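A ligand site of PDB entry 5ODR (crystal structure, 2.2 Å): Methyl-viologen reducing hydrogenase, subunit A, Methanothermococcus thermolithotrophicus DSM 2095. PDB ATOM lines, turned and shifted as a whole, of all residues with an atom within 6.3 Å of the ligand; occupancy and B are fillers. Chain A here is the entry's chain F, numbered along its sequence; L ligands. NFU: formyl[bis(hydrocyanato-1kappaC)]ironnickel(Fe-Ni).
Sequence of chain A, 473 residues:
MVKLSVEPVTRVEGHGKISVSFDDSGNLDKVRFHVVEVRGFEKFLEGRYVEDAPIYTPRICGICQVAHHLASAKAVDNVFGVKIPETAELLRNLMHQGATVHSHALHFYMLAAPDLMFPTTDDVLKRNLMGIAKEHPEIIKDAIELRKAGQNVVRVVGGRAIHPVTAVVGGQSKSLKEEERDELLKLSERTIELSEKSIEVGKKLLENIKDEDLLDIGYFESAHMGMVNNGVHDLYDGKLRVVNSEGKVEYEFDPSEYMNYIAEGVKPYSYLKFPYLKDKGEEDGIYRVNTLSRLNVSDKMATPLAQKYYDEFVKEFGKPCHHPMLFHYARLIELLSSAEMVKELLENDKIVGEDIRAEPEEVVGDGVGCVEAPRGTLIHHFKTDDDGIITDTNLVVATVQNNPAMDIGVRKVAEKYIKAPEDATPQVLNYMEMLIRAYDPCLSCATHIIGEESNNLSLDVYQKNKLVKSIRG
The side-chain sulfur (SG) of Cys 61 binds a nickel atom (NI) of the ligand (2.2 Å).
A nitrogen (N2) of the ligand sits at hydrogen-bond distance from the side-chain hydroxyl (OG1) of Thr 399 (3.1 Å).
NI of the ligand is bound by SG of Cys 442.
N1 of the ligand lies within hydrogen-bond range of N of Arg 375.
N of Thr 399 sits at hydrogen-bond distance from N2 of the ligand, 3.3 Å away.
NH1 of Arg 375 sits at hydrogen-bond distance from N1 of the ligand (3.1 Å).
A nickel atom (NI) of the ligand is bound by the side-chain sulfur of Cys 64 (2.2 Å).
SG of Cys 445 is bound to FE of the ligand.
SG of Cys 61 sits close to N of Ile 63, at 3.3 Å.
NH1 of Arg 375 is in hydrogen-bond range of OG of Ser 103, at 2.7 Å.
OE1 of Glu 13 lies close to SG of Cys 442 (3.2 Å).
The side-chain carboxylate (OD1) of Asp 440 lies within salt-bridge range of the guanidinium group (NE) of Arg 375.
The backbone carbonyl oxygen of Thr 377 lies within hydrogen-bond range of the backbone NH of Ala 398 (3.1 Å).
The side-chain sulfur (SG) of Cys 445 sits close to a ring nitrogen (NE2) of His 68 (2.9 Å).
OG1 of Thr 399 sits at hydrogen-bond distance from N of Cys 442.
ND1 of His 68 sits at hydrogen-bond distance from NE2 of His 380, at 2.9 Å.
N1 of the ligand sits close to N of Pro 374 (3.5 Å).
NE2 of His 68 touches C3 of the ligand, 3.6 Å away.
Ala 373 touches the ligand.
Leu 378 touches the ligand (CD2 to O3, 3.2 Å).
Val 397 touches the ligand (CG1 to O3, 3.5 Å).
CB of Ala 398 touches N2 of the ligand, at 3.7 Å.
Within 4 Å of the ligand: Cys 61, Cys 64, His 68, Ala 373, Pro 374, Arg 375, Leu 378, Val 397, Ala 398, Thr 399, Cys 442 and Cys 445.
Along chain A the residues within 4 Å of the ligand span positions 61 to 445.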
ATOM      1  N   GLU A  13      24.864   8.336  26.002  1.00  0.00           N
ATOM      2  CA  GLU A  13      24.233   9.182  26.989  1.00  0.00           C
ATOM      3  C   GLU A  13      22.843   8.586  27.212  1.00  0.00           C
ATOM      4  O   GLU A  13      22.152   8.285  26.255  1.00  0.00           O
ATOM      5  CB  GLU A  13      24.110  10.645  26.519  1.00  0.00           C
ATOM      6  CG  GLU A  13      23.504  11.574  27.565  1.00  0.00           C
ATOM      7  CD  GLU A  13      22.056  11.282  27.929  1.00  0.00           C
ATOM      8  OE1 GLU A  13      21.250  11.040  27.007  1.00  0.00           O
ATOM      9  OE2 GLU A  13      21.756  11.245  29.144  1.00  0.00           O
ATOM     10  N   ILE A  60      16.771  18.905  29.379  1.00  0.00           N
ATOM     11  CA  ILE A  60      16.404  17.661  28.705  1.00  0.00           C
ATOM     12  C   ILE A  60      17.736  16.903  28.562  1.00  0.00           C
ATOM     13  O   ILE A  60      17.760  15.678  28.655  1.00  0.00           O
ATOM     14  CB  ILE A  60      15.771  17.914  27.315  1.00  0.00           C
ATOM     15  CG1 ILE A  60      14.331  18.424  27.446  1.00  0.00           C
ATOM     16  CG2 ILE A  60      15.818  16.653  26.452  1.00  0.00           C
ATOM     17  CD1 ILE A  60      13.767  19.004  26.173  1.00  0.00           C
ATOM     18  N   CYS A  61      18.855  17.630  28.326  1.00  0.00           N
ATOM     19  CA  CYS A  61      20.153  16.981  28.159  1.00  0.00           C
ATOM     20  C   CYS A  61      21.338  17.886  28.510  1.00  0.00           C
ATOM     21  O   CYS A  61      21.401  19.037  28.092  1.00  0.00           O
ATOM     22  CB  CYS A  61      20.288  16.452  26.740  1.00  0.00           C
ATOM     23  SG  CYS A  61      21.921  15.779  26.370  1.00  0.00           S
ATOM     24  N   GLY A  62      22.269  17.334  29.275  1.00  0.00           N
ATOM     25  CA  GLY A  62      23.468  18.033  29.716  1.00  0.00           C
ATOM     26  C   GLY A  62      24.580  18.156  28.693  1.00  0.00           C
ATOM     27  O   GLY A  62      25.525  18.905  28.915  1.00  0.00           O
ATOM     28  N   ILE A  63      24.475  17.431  27.558  1.00  0.00           N
ATOM     29  CA  ILE A  63      25.489  17.502  26.501  1.00  0.00           C
ATOM     30  C   ILE A  63      25.090  18.533  25.453  1.00  0.00           C
ATOM     31  O   ILE A  63      25.856  19.442  25.142  1.00  0.00           O
ATOM     32  CB  ILE A  63      25.682  16.128  25.819  1.00  0.00           C
ATOM     33  CG1 ILE A  63      26.253  15.092  26.809  1.00  0.00           C
ATOM     34  CG2 ILE A  63      26.595  16.268  24.606  1.00  0.00           C
ATOM     35  CD1 ILE A  63      26.211  13.625  26.275  1.00  0.00           C
ATOM     36  N   CYS A  64      23.875  18.386  24.915  1.00  0.00           N
ATOM     37  CA  CYS A  64      23.332  19.262  23.879  1.00  0.00           C
ATOM     38  C   CYS A  64      22.355  20.302  24.443  1.00  0.00           C
ATOM     39  O   CYS A  64      21.376  20.637  23.770  1.00  0.00           O
ATOM     40  CB  CYS A  64      22.639  18.394  22.835  1.00  0.00           C
ATOM     41  SG  CYS A  64      21.190  17.525  23.478  1.00  0.00           S
ATOM     42  N   GLN A  65      22.613  20.824  25.638  1.00  0.00           N
ATOM     43  CA  GLN A  65      21.711  21.821  26.234  1.00  0.00           C
ATOM     44  C   GLN A  65      21.661  23.106  25.409  1.00  0.00           C
ATOM     45  O   GLN A  65      20.639  23.799  25.423  1.00  0.00           O
ATOM     46  CB  GLN A  65      22.060  22.155  27.705  1.00  0.00           C
ATOM     47  CG  GLN A  65      23.303  21.488  28.287  1.00  0.00           C
ATOM     48  CD  GLN A  65      24.581  22.138  27.823  1.00  0.00           C
ATOM     49  OE1 GLN A  65      24.610  23.332  27.522  1.00  0.00           O
ATOM     50  NE2 GLN A  65      25.666  21.385  27.814  1.00  0.00           N
ATOM     51  N   ALA A  67      21.714  23.359  22.073  1.00  0.00           N
ATOM     52  CA  ALA A  67      20.760  23.127  20.991  1.00  0.00           C
ATOM     53  C   ALA A  67      19.327  23.369  21.472  1.00  0.00           C
ATOM     54  O   ALA A  67      18.556  24.006  20.785  1.00  0.00           O
ATOM     55  CB  ALA A  67      20.933  21.713  20.449  1.00  0.00           C
ATOM     56  N   HIS A  68      18.984  22.856  22.672  1.00  0.00           N
ATOM     57  CA  HIS A  68      17.635  23.033  23.239  1.00  0.00           C
ATOM     58  C   HIS A  68      17.372  24.483  23.586  1.00  0.00           C
ATOM     59  O   HIS A  68      16.289  24.996  23.285  1.00  0.00           O
ATOM     60  CB  HIS A  68      17.453  22.154  24.474  1.00  0.00           C
ATOM     61  CG  HIS A  68      17.360  20.704  24.149  1.00  0.00           C
ATOM     62  ND1 HIS A  68      16.281  20.187  23.455  1.00  0.00           N
ATOM     63  CD2 HIS A  68      18.212  19.697  24.447  1.00  0.00           C
ATOM     64  CE1 HIS A  68      16.507  18.892  23.342  1.00  0.00           C
ATOM     65  NE2 HIS A  68      17.651  18.545  23.926  1.00  0.00           N
ATOM     66  N   SER A 103      30.561  18.653  21.875  1.00  0.00           N
ATOM     67  CA  SER A 103      29.792  17.424  21.736  1.00  0.00           C
ATOM     68  C   SER A 103      30.469  16.399  20.831  1.00  0.00           C
ATOM     69  O   SER A 103      30.589  15.238  21.220  1.00  0.00           O
ATOM     70  CB  SER A 103      28.389  17.739  21.237  1.00  0.00           C
ATOM     71  OG  SER A 103      27.563  16.592  21.271  1.00  0.00           O
ATOM     72  N   ALA A 373      20.851  19.755  16.021  1.00  0.00           N
ATOM     73  CA  ALA A 373      21.586  19.507  17.241  1.00  0.00           C
ATOM     74  C   ALA A 373      22.742  18.591  16.820  1.00  0.00           C
ATOM     75  O   ALA A 373      22.662  17.970  15.765  1.00  0.00           O
ATOM     76  CB  ALA A 373      20.700  18.813  18.260  1.00  0.00           C
ATOM     77  N   PRO A 374      23.818  18.466  17.605  1.00  0.00           N
ATOM     78  CA  PRO A 374      24.914  17.575  17.157  1.00  0.00           C
ATOM     79  C   PRO A 374      24.479  16.151  16.786  1.00  0.00           C
ATOM     80  O   PRO A 374      25.170  15.485  16.025  1.00  0.00           O
ATOM     81  CB  PRO A 374      25.868  17.561  18.363  1.00  0.00           C
ATOM     82  CG  PRO A 374      25.578  18.809  19.109  1.00  0.00           C
ATOM     83  CD  PRO A 374      24.121  19.111  18.891  1.00  0.00           C
ATOM     84  N   ARG A 375      23.325  15.687  17.314  1.00  0.00           N
ATOM     85  CA  ARG A 375      22.823  14.343  17.041  1.00  0.00           C
ATOM     86  C   ARG A 375      21.646  14.286  16.087  1.00  0.00           C
ATOM     87  O   ARG A 375      20.999  13.237  15.992  1.00  0.00           O
ATOM     88  CB  ARG A 375      22.501  13.639  18.348  1.00  0.00           C
ATOM     89  CG  ARG A 375      23.757  13.404  19.125  1.00  0.00           C
ATOM     90  CD  ARG A 375      23.556  13.115  20.594  1.00  0.00           C
ATOM     91  NE  ARG A 375      24.859  12.911  21.217  1.00  0.00           N
ATOM     92  CZ  ARG A 375      25.680  13.887  21.601  1.00  0.00           C
ATOM     93  NH1 ARG A 375      25.314  15.153  21.438  1.00  0.00           N
ATOM     94  NH2 ARG A 375      26.847  13.609  22.145  1.00  0.00           N
ATOM     95  N   GLY A 376      21.369  15.371  15.378  1.00  0.00           N
ATOM     96  CA  GLY A 376      20.276  15.408  14.416  1.00  0.00           C
ATOM     97  C   GLY A 376      19.362  16.587  14.535  1.00  0.00           C
ATOM     98  O   GLY A 376      19.533  17.449  15.406  1.00  0.00           O
ATOM     99  N   THR A 377      18.366  16.640  13.633  1.00  0.00           N
ATOM    100  CA  THR A 377      17.369  17.698  13.580  1.00  0.00           C
ATOM    101  C   THR A 377      16.629  17.817  14.894  1.00  0.00           C
ATOM    102  O   THR A 377      16.133  16.811  15.421  1.00  0.00           O
ATOM    103  CB  THR A 377      16.379  17.439  12.439  1.00  0.00           C
ATOM    104  OG1 THR A 377      17.109  17.087  11.264  1.00  0.00           O
ATOM    105  CG2 THR A 377      15.501  18.643  12.160  1.00  0.00           C
ATOM    106  N   LEU A 378      16.563  19.029  15.429  1.00  0.00           N
ATOM    107  CA  LEU A 378      15.895  19.305  16.691  1.00  0.00           C
ATOM    108  C   LEU A 378      14.756  20.268  16.438  1.00  0.00           C
ATOM    109  O   LEU A 378      14.980  21.348  15.904  1.00  0.00           O
ATOM    110  CB  LEU A 378      16.883  19.910  17.678  1.00  0.00           C
ATOM    111  CG  LEU A 378      16.310  20.361  19.021  1.00  0.00           C
ATOM    112  CD1 LEU A 378      15.578  19.217  19.711  1.00  0.00           C
ATOM    113  CD2 LEU A 378      17.404  20.907  19.898  1.00  0.00           C
ATOM    114  N   HIS A 380      11.429  22.202  18.335  1.00  0.00           N
ATOM    115  CA  HIS A 380      10.708  22.577  19.548  1.00  0.00           C
ATOM    116  C   HIS A 380       9.468  23.309  19.039  1.00  0.00           C
ATOM    117  O   HIS A 380       9.612  24.333  18.371  1.00  0.00           O
ATOM    118  CB  HIS A 380      11.547  23.523  20.426  1.00  0.00           C
ATOM    119  CG  HIS A 380      12.623  22.852  21.236  1.00  0.00           C
ATOM    120  ND1 HIS A 380      13.193  23.489  22.321  1.00  0.00           N
ATOM    121  CD2 HIS A 380      13.186  21.633  21.105  1.00  0.00           C
ATOM    122  CE1 HIS A 380      14.088  22.646  22.810  1.00  0.00           C
ATOM    123  NE2 HIS A 380      14.116  21.516  22.117  1.00  0.00           N
ATOM    124  N   VAL A 396      10.559  16.984  18.779  1.00  0.00           N
ATOM    125  CA  VAL A 396      11.064  15.913  17.902  1.00  0.00           C
ATOM    126  C   VAL A 396      12.564  16.100  18.111  1.00  0.00           C
ATOM    127  O   VAL A 396      13.183  16.972  17.495  1.00  0.00           O
ATOM    128  CB  VAL A 396      10.643  16.090  16.427  1.00  0.00           C
ATOM    129  CG1 VAL A 396      11.182  14.945  15.572  1.00  0.00           C
ATOM    130  CG2 VAL A 396       9.128  16.186  16.315  1.00  0.00           C
ATOM    131  N   VAL A 397      13.121  15.299  19.020  1.00  0.00           N
ATOM    132  CA  VAL A 397      14.518  15.424  19.404  1.00  0.00           C
ATOM    133  C   VAL A 397      15.526  14.446  18.829  1.00  0.00           C
ATOM    134  O   VAL A 397      15.641  13.292  19.254  1.00  0.00           O
ATOM    135  CB  VAL A 397      14.590  15.399  20.952  1.00  0.00           C
ATOM    136  CG1 VAL A 397      16.005  15.690  21.438  1.00  0.00           C
ATOM    137  CG2 VAL A 397      13.604  16.408  21.548  1.00  0.00           C
ATOM    138  N   ALA A 398      16.298  14.976  17.874  1.00  0.00           N
ATOM    139  CA  ALA A 398      17.396  14.346  17.163  1.00  0.00           C
ATOM    140  C   ALA A 398      17.466  12.799  17.202  1.00  0.00           C
ATOM    141  O   ALA A 398      16.884  12.158  16.329  1.00  0.00           O
ATOM    142  CB  ALA A 398      18.685  14.945  17.702  1.00  0.00           C
ATOM    143  N   THR A 399      18.181  12.192  18.179  1.00  0.00           N
ATOM    144  CA  THR A 399      18.339  10.732  18.288  1.00  0.00           C
ATOM    145  C   THR A 399      17.062   9.909  18.093  1.00  0.00           C
ATOM    146  O   THR A 399      17.175   8.784  17.627  1.00  0.00           O
ATOM    147  CB  THR A 399      19.049  10.364  19.601  1.00  0.00           C
ATOM    148  OG1 THR A 399      20.444  10.651  19.447  1.00  0.00           O
ATOM    149  CG2 THR A 399      18.899   8.882  19.958  1.00  0.00           C
ATOM    150  N   VAL A 400      15.872  10.432  18.441  1.00  0.00           N
ATOM    151  CA  VAL A 400      14.644   9.639  18.240  1.00  0.00           C
ATOM    152  C   VAL A 400      14.550   9.185  16.790  1.00  0.00           C
ATOM    153  O   VAL A 400      14.120   8.069  16.515  1.00  0.00           O
ATOM    154  CB  VAL A 400      13.354  10.388  18.691  1.00  0.00           C
ATOM    155  CG1 VAL A 400      13.081  11.619  17.831  1.00  0.00           C
ATOM    156  CG2 VAL A 400      12.143   9.467  18.685  1.00  0.00           C
ATOM    157  N   ASP A 440      25.967   8.079  17.968  1.00  0.00           N
ATOM    158  CA  ASP A 440      26.122   9.051  19.054  1.00  0.00           C
ATOM    159  C   ASP A 440      24.751   9.280  19.686  1.00  0.00           C
ATOM    160  O   ASP A 440      24.253  10.404  19.710  1.00  0.00           O
ATOM    161  CB  ASP A 440      26.728  10.372  18.520  1.00  0.00           C
ATOM    162  CG  ASP A 440      27.070  11.406  19.580  1.00  0.00           C
ATOM    163  OD1 ASP A 440      27.010  11.059  20.783  1.00  0.00           O
ATOM    164  OD2 ASP A 440      27.414  12.542  19.204  1.00  0.00           O
ATOM    165  N   PRO A 441      24.100   8.224  20.198  1.00  0.00           N
ATOM    166  CA  PRO A 441      22.780   8.419  20.793  1.00  0.00           C
ATOM    167  C   PRO A 441      22.769   9.136  22.129  1.00  0.00           C
ATOM    168  O   PRO A 441      23.673   8.959  22.955  1.00  0.00           O
ATOM    169  CB  PRO A 441      22.249   6.994  20.942  1.00  0.00           C
ATOM    170  CG  PRO A 441      23.462   6.161  21.076  1.00  0.00           C
ATOM    171  CD  PRO A 441      24.521   6.819  20.251  1.00  0.00           C
ATOM    172  N   CYS A 442      21.734   9.940  22.334  1.00  0.00           N
ATOM    173  CA  CYS A 442      21.499  10.704  23.548  1.00  0.00           C
ATOM    174  C   CYS A 442      20.078  10.295  23.908  1.00  0.00           C
ATOM    175  O   CYS A 442      19.109  10.909  23.478  1.00  0.00           O
ATOM    176  CB  CYS A 442      21.631  12.203  23.267  1.00  0.00           C
ATOM    177  SG  CYS A 442      21.747  13.236  24.745  1.00  0.00           S
ATOM    178  N   LEU A 443      19.980   9.213  24.682  1.00  0.00           N
ATOM    179  CA  LEU A 443      18.705   8.621  25.082  1.00  0.00           C
ATOM    180  C   LEU A 443      17.841   9.477  26.023  1.00  0.00           C
ATOM    181  O   LEU A 443      16.620   9.323  26.002  1.00  0.00           O
ATOM    182  CB  LEU A 443      18.943   7.214  25.645  1.00  0.00           C
ATOM    183  CG  LEU A 443      19.809   6.301  24.719  1.00  0.00           C
ATOM    184  CD1 LEU A 443      20.104   4.975  25.381  1.00  0.00           C
ATOM    185  CD2 LEU A 443      19.146   6.096  23.373  1.00  0.00           C
ATOM    186  N   SER A 444      18.436  10.380  26.831  1.00  0.00           N
ATOM    187  CA  SER A 444      17.636  11.247  27.714  1.00  0.00           C
ATOM    188  C   SER A 444      16.945  12.261  26.826  1.00  0.00           C
ATOM    189  O   SER A 444      15.787  12.619  27.000  1.00  0.00           O
ATOM    190  CB  SER A 444      18.546  11.989  28.709  1.00  0.00           C
ATOM    191  OG  SER A 444      18.985  11.130  29.754  1.00  0.00           O
ATOM    192  N   CYS A 445      17.702  12.708  25.830  1.00  0.00           N
ATOM    193  CA  CYS A 445      17.286  13.672  24.831  1.00  0.00           C
ATOM    194  C   CYS A 445      16.161  13.134  23.959  1.00  0.00           C
ATOM    195  O   CYS A 445      15.134  13.786  23.774  1.00  0.00           O
ATOM    196  CB  CYS A 445      18.485  14.032  23.968  1.00  0.00           C
ATOM    197  SG  CYS A 445      18.665  15.792  23.639  1.00  0.00           S
ATOM    198  N   ALA A 446      16.372  11.942  23.412  1.00  0.00           N
ATOM    199  CA  ALA A 446      15.432  11.280  22.507  1.00  0.00           C
ATOM    200  C   ALA A 446      14.039  11.039  23.077  1.00  0.00           C
ATOM    201  O   ALA A 446      13.065  11.124  22.343  1.00  0.00           O
ATOM    202  CB  ALA A 446      16.042   9.979  22.038  1.00  0.00           C
HETATM  203 FE   NFU L   1      20.339  16.088  21.931  1.00  0.00          FE
HETATM  204 NI   NFU L   1      21.520  15.435  24.199  1.00  0.00          NI
HETATM  205  C1  NFU L   1      21.825  16.286  20.881  1.00  0.00           C
HETATM  206  N1  NFU L   1      22.736  16.449  20.202  1.00  0.00           N
HETATM  207  C2  NFU L   1      20.115  14.417  21.239  1.00  0.00           C
HETATM  208  N2  NFU L   1      19.921  13.389  20.771  1.00  0.00           N
HETATM  209  C3  NFU L   1      19.236  17.193  20.995  1.00  0.00           C
HETATM  210  O3  NFU L   1      18.497  17.908  20.364  1.00  0.00           O
